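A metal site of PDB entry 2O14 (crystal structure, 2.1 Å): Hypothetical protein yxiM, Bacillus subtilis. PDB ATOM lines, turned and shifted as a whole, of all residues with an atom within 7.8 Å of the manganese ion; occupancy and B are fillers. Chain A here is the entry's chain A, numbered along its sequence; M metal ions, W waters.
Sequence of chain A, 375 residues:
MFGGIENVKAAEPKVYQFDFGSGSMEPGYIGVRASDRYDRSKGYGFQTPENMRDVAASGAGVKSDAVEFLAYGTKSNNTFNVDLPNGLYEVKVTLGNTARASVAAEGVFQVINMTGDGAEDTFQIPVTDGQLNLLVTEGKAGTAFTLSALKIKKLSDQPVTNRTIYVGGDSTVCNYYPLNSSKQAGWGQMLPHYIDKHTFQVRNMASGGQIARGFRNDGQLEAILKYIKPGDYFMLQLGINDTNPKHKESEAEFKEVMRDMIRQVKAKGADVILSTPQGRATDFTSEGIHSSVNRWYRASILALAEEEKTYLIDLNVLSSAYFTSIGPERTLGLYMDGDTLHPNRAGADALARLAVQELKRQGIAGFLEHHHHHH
OG of Ser 24 sits at hydrogen-bond distance from OE2 of Glu 26.
N of Glu 26 sits close to OD2 of Asp 19 (3.2 Å).
The backbone carbonyl oxygen of Asp 19 is in hydrogen-bond range of the backbone NH of Val 32 (3.0 Å).
The backbone NH (N) of Asp 19 lies within hydrogen-bond range of the backbone carbonyl oxygen (O) of Ile 30 (2.8 Å).
The backbone NH of Gly 23 lies close to the side-chain carboxylate of Asp 65.
The backbone carbonyl oxygen of Asp 65 is in hydrogen-bond range of the side-chain hydroxyl of Ser 148.
N of Phe 20 lies within hydrogen-bond range of O of Ser 148, 2.9 Å away.
The backbone carbonyl oxygen (O) of Phe 20 lies close to the backbone NH (N) of Ala 66.
Phe 20 touches the manganese ion.
Within 4 Å of the manganese ion: Asp 19, Phe 20, Ser 24 and Asp 65.
The manganese ion is bound by O of Ser 24 (2.1 Å), water W2 (2.2 Å), OD2 of Asp 19 (2.3 Å), OD1 of Asp 65 (2.3 Å), water W1 (2.3 Å), OD2 of Asp 65 (2.4 Å) and OD1 of Asp 19 (2.4 Å).
The manganese ion has seven donor atoms within binding distance.
Water W2 lies within hydrogen-bond range of OE2 of Glu 26 (2.9 Å), O of Gly 61 (3.0 Å) and OG of Ser 64 (3.1 Å).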
ATOM      1  N   PHE A  18     -13.547  20.264  -7.467  1.00  0.00           N
ATOM      2  CA  PHE A  18     -12.712  20.950  -8.437  1.00  0.00           C
ATOM      3  C   PHE A  18     -12.931  22.458  -8.422  1.00  0.00           C
ATOM      4  O   PHE A  18     -14.062  22.925  -8.470  1.00  0.00           O
ATOM      5  CB  PHE A  18     -13.006  20.394  -9.840  1.00  0.00           C
ATOM      6  CG  PHE A  18     -12.761  18.921  -9.965  1.00  0.00           C
ATOM      7  CD1 PHE A  18     -11.458  18.417 -10.019  1.00  0.00           C
ATOM      8  CD2 PHE A  18     -13.820  18.015  -9.984  1.00  0.00           C
ATOM      9  CE1 PHE A  18     -11.219  17.046 -10.106  1.00  0.00           C
ATOM     10  CE2 PHE A  18     -13.594  16.641 -10.073  1.00  0.00           C
ATOM     11  CZ  PHE A  18     -12.293  16.147 -10.127  1.00  0.00           C
ATOM     12  N   ASP A  19     -11.842  23.198  -8.337  1.00  0.00           N
ATOM     13  CA  ASP A  19     -11.879  24.661  -8.344  1.00  0.00           C
ATOM     14  C   ASP A  19     -11.283  25.079  -9.683  1.00  0.00           C
ATOM     15  O   ASP A  19     -10.064  25.077  -9.867  1.00  0.00           O
ATOM     16  CB  ASP A  19     -11.047  25.226  -7.180  1.00  0.00           C
ATOM     17  CG  ASP A  19     -10.801  26.727  -7.303  1.00  0.00           C
ATOM     18  OD1 ASP A  19     -11.599  27.401  -7.972  1.00  0.00           O
ATOM     19  OD2 ASP A  19      -9.823  27.235  -6.712  1.00  0.00           O
ATOM     20  N   PHE A  20     -12.149  25.429 -10.621  1.00  0.00           N
ATOM     21  CA  PHE A  20     -11.739  25.828 -11.963  1.00  0.00           C
ATOM     22  C   PHE A  20     -11.201  27.248 -12.068  1.00  0.00           C
ATOM     23  O   PHE A  20     -11.749  28.181 -11.477  1.00  0.00           O
ATOM     24  CB  PHE A  20     -12.915  25.653 -12.923  1.00  0.00           C
ATOM     25  CG  PHE A  20     -13.357  24.221 -13.067  1.00  0.00           C
ATOM     26  CD1 PHE A  20     -12.713  23.365 -13.971  1.00  0.00           C
ATOM     27  CD2 PHE A  20     -14.403  23.713 -12.286  1.00  0.00           C
ATOM     28  CE1 PHE A  20     -13.100  22.026 -14.082  1.00  0.00           C
ATOM     29  CE2 PHE A  20     -14.797  22.373 -12.391  1.00  0.00           C
ATOM     30  CZ  PHE A  20     -14.148  21.529 -13.301  1.00  0.00           C
ATOM     31  N   GLY A  21     -10.134  27.412 -12.847  1.00  0.00           N
ATOM     32  CA  GLY A  21      -9.532  28.722 -13.016  1.00  0.00           C
ATOM     33  C   GLY A  21      -8.054  28.699 -12.678  1.00  0.00           C
ATOM     34  O   GLY A  21      -7.558  27.715 -12.132  1.00  0.00           O
ATOM     35  N   SER A  22      -7.339  29.775 -12.998  1.00  0.00           N
ATOM     36  CA  SER A  22      -5.907  29.843 -12.715  1.00  0.00           C
ATOM     37  C   SER A  22      -5.502  30.940 -11.732  1.00  0.00           C
ATOM     38  O   SER A  22      -4.323  31.047 -11.390  1.00  0.00           O
ATOM     39  CB  SER A  22      -5.135  30.032 -14.031  1.00  0.00           C
ATOM     40  OG  SER A  22      -5.540  31.228 -14.685  1.00  0.00           O
ATOM     41  N   GLY A  23      -6.455  31.746 -11.269  1.00  0.00           N
ATOM     42  CA  GLY A  23      -6.107  32.820 -10.352  1.00  0.00           C
ATOM     43  C   GLY A  23      -5.737  32.391  -8.946  1.00  0.00           C
ATOM     44  O   GLY A  23      -4.669  32.743  -8.430  1.00  0.00           O
ATOM     45  N   SER A  24      -6.621  31.629  -8.323  1.00  0.00           N
ATOM     46  CA  SER A  24      -6.408  31.146  -6.959  1.00  0.00           C
ATOM     47  C   SER A  24      -6.918  29.702  -6.821  1.00  0.00           C
ATOM     48  O   SER A  24      -7.858  29.294  -7.504  1.00  0.00           O
ATOM     49  CB  SER A  24      -7.155  32.073  -5.970  1.00  0.00           C
ATOM     50  OG  SER A  24      -6.868  31.759  -4.611  1.00  0.00           O
ATOM     51  N   MET A  25      -6.250  28.932  -5.962  1.00  0.00           N
ATOM     52  CA  MET A  25      -6.633  27.546  -5.701  1.00  0.00           C
ATOM     53  C   MET A  25      -6.990  27.446  -4.221  1.00  0.00           C
ATOM     54  O   MET A  25      -6.149  27.682  -3.344  1.00  0.00           O
ATOM     55  CB  MET A  25      -5.473  26.601  -6.040  1.00  0.00           C
ATOM     56  CG  MET A  25      -5.228  26.381  -7.539  1.00  0.00           C
ATOM     57  SD  MET A  25      -4.488  27.895  -8.548  1.00  0.00           S
ATOM     58  CE  MET A  25      -2.649  27.288  -8.737  1.00  0.00           C
ATOM     59  N   GLU A  26      -8.244  27.114  -3.936  1.00  0.00           N
ATOM     60  CA  GLU A  26      -8.724  27.028  -2.569  1.00  0.00           C
ATOM     61  C   GLU A  26      -8.546  25.651  -1.950  1.00  0.00           C
ATOM     62  O   GLU A  26      -8.684  24.624  -2.614  1.00  0.00           O
ATOM     63  CB  GLU A  26     -10.199  27.435  -2.503  1.00  0.00           C
ATOM     64  CG  GLU A  26     -10.545  28.734  -3.239  1.00  0.00           C
ATOM     65  CD  GLU A  26      -9.520  29.840  -3.020  1.00  0.00           C
ATOM     66  OE1 GLU A  26      -9.033  30.015  -1.888  1.00  0.00           O
ATOM     67  OE2 GLU A  26      -9.211  30.559  -3.998  1.00  0.00           O
ATOM     68  N   TYR A  29      -9.981  21.748  -2.528  1.00  0.00           N
ATOM     69  CA  TYR A  29     -10.356  21.675  -3.926  1.00  0.00           C
ATOM     70  C   TYR A  29      -9.148  21.378  -4.793  1.00  0.00           C
ATOM     71  O   TYR A  29      -8.045  21.816  -4.499  1.00  0.00           O
ATOM     72  CB  TYR A  29     -10.932  23.011  -4.397  1.00  0.00           C
ATOM     73  CG  TYR A  29     -12.350  23.300  -3.960  1.00  0.00           C
ATOM     74  CD1 TYR A  29     -13.417  23.037  -4.810  1.00  0.00           C
ATOM     75  CD2 TYR A  29     -12.620  23.880  -2.721  1.00  0.00           C
ATOM     76  CE1 TYR A  29     -14.732  23.337  -4.434  1.00  0.00           C
ATOM     77  CE2 TYR A  29     -13.916  24.184  -2.334  1.00  0.00           C
ATOM     78  CZ  TYR A  29     -14.964  23.915  -3.196  1.00  0.00           C
ATOM     79  OH  TYR A  29     -16.255  24.220  -2.837  1.00  0.00           O
ATOM     80  N   ILE A  30      -9.378  20.634  -5.868  1.00  0.00           N
ATOM     81  CA  ILE A  30      -8.305  20.348  -6.815  1.00  0.00           C
ATOM     82  C   ILE A  30      -8.411  21.470  -7.838  1.00  0.00           C
ATOM     83  O   ILE A  30      -9.470  21.671  -8.446  1.00  0.00           O
ATOM     84  CB  ILE A  30      -8.507  19.021  -7.548  1.00  0.00           C
ATOM     85  CG1 ILE A  30      -8.293  17.850  -6.580  1.00  0.00           C
ATOM     86  CG2 ILE A  30      -7.545  18.935  -8.731  1.00  0.00           C
ATOM     87  CD1 ILE A  30      -8.511  16.500  -7.238  1.00  0.00           C
ATOM     88  N   GLY A  31      -7.333  22.226  -8.005  1.00  0.00           N
ATOM     89  CA  GLY A  31      -7.345  23.307  -8.963  1.00  0.00           C
ATOM     90  C   GLY A  31      -7.278  22.744 -10.371  1.00  0.00           C
ATOM     91  O   GLY A  31      -6.411  21.932 -10.663  1.00  0.00           O
ATOM     92  N   VAL A  32      -8.193  23.166 -11.238  1.00  0.00           N
ATOM     93  CA  VAL A  32      -8.202  22.701 -12.620  1.00  0.00           C
ATOM     94  C   VAL A  32      -8.171  23.914 -13.531  1.00  0.00           C
ATOM     95  O   VAL A  32      -9.075  24.756 -13.525  1.00  0.00           O
ATOM     96  CB  VAL A  32      -9.440  21.845 -12.940  1.00  0.00           C
ATOM     97  CG1 VAL A  32      -9.319  21.284 -14.361  1.00  0.00           C
ATOM     98  CG2 VAL A  32      -9.571  20.714 -11.935  1.00  0.00           C
ATOM     99  N   GLY A  61     -13.666  33.120  -2.970  1.00  0.00           N
ATOM    100  CA  GLY A  61     -13.233  31.729  -2.968  1.00  0.00           C
ATOM    101  C   GLY A  61     -13.172  31.145  -4.356  1.00  0.00           C
ATOM    102  O   GLY A  61     -12.693  31.787  -5.293  1.00  0.00           O
ATOM    103  N   VAL A  62     -13.662  29.916  -4.510  1.00  0.00           N
ATOM    104  CA  VAL A  62     -13.644  29.263  -5.821  1.00  0.00           C
ATOM    105  C   VAL A  62     -14.424  30.039  -6.885  1.00  0.00           C
ATOM    106  O   VAL A  62     -14.314  29.753  -8.072  1.00  0.00           O
ATOM    107  CB  VAL A  62     -14.192  27.821  -5.718  1.00  0.00           C
ATOM    108  CG1 VAL A  62     -13.285  26.998  -4.820  1.00  0.00           C
ATOM    109  CG2 VAL A  62     -15.610  27.825  -5.187  1.00  0.00           C
ATOM    110  N   LYS A  63     -15.200  31.035  -6.452  1.00  0.00           N
ATOM    111  CA  LYS A  63     -16.000  31.849  -7.361  1.00  0.00           C
ATOM    112  C   LYS A  63     -15.207  33.042  -7.903  1.00  0.00           C
ATOM    113  O   LYS A  63     -15.743  33.830  -8.697  1.00  0.00           O
ATOM    114  CB  LYS A  63     -17.265  32.337  -6.656  1.00  0.00           C
ATOM    115  CG  LYS A  63     -18.199  31.226  -6.251  1.00  0.00           C
ATOM    116  CD  LYS A  63     -19.493  31.778  -5.671  1.00  0.00           C
ATOM    117  CE  LYS A  63     -20.431  30.676  -5.252  1.00  0.00           C
ATOM    118  NZ  LYS A  63     -21.686  31.246  -4.701  1.00  0.00           N
ATOM    119  N   SER A  64     -13.960  33.175  -7.477  1.00  0.00           N
ATOM    120  CA  SER A  64     -13.103  34.269  -7.924  1.00  0.00           C
ATOM    121  C   SER A  64     -12.517  34.010  -9.310  1.00  0.00           C
ATOM    122  O   SER A  64     -11.991  34.921  -9.953  1.00  0.00           O
ATOM    123  CB  SER A  64     -11.956  34.479  -6.925  1.00  0.00           C
ATOM    124  OG  SER A  64     -11.051  33.391  -7.016  1.00  0.00           O
ATOM    125  N   ASP A  65     -12.570  32.758  -9.766  1.00  0.00           N
ATOM    126  CA  ASP A  65     -12.033  32.428 -11.083  1.00  0.00           C
ATOM    127  C   ASP A  65     -12.819  31.306 -11.736  1.00  0.00           C
ATOM    128  O   ASP A  65     -13.628  30.652 -11.083  1.00  0.00           O
ATOM    129  CB  ASP A  65     -10.543  32.057 -10.980  1.00  0.00           C
ATOM    130  CG  ASP A  65     -10.283  30.926  -9.989  1.00  0.00           C
ATOM    131  OD1 ASP A  65     -11.248  30.382  -9.418  1.00  0.00           O
ATOM    132  OD2 ASP A  65      -9.102  30.583  -9.787  1.00  0.00           O
ATOM    133  N   ALA A  66     -12.572  31.079 -13.027  1.00  0.00           N
ATOM    134  CA  ALA A  66     -13.289  30.032 -13.752  1.00  0.00           C
ATOM    135  C   ALA A  66     -12.660  29.710 -15.097  1.00  0.00           C
ATOM    136  O   ALA A  66     -11.642  30.288 -15.465  1.00  0.00           O
ATOM    137  CB  ALA A  66     -14.739  30.471 -13.954  1.00  0.00           C
ATOM    138  N   SER A 148     -16.981  27.770 -12.379  1.00  0.00           N
ATOM    139  CA  SER A 148     -16.061  28.076 -11.286  1.00  0.00           C
ATOM    140  C   SER A 148     -15.719  26.869 -10.427  1.00  0.00           C
ATOM    141  O   SER A 148     -14.602  26.751  -9.957  1.00  0.00           O
ATOM    142  CB  SER A 148     -16.625  29.173 -10.378  1.00  0.00           C
ATOM    143  OG  SER A 148     -16.446  30.472 -10.926  1.00  0.00           O
ATOM    144  N   ALA A 149     -16.680  25.996 -10.199  1.00  0.00           N
ATOM    145  CA  ALA A 149     -16.402  24.837  -9.364  1.00  0.00           C
ATOM    146  C   ALA A 149     -17.383  23.689  -9.534  1.00  0.00           C
ATOM    147  O   ALA A 149     -18.476  23.873 -10.056  1.00  0.00           O
ATOM    148  CB  ALA A 149     -16.383  25.254  -7.895  1.00  0.00           C
HETATM  149 MN    MN M   1      -9.840  29.035  -8.148  1.00  0.00          MN
HETATM  150  O   HOH W   1      -8.923  27.384  -9.535  1.00  0.00           O
HETATM  151  O   HOH W   2     -10.421  30.421  -6.597  1.00  0.00           O
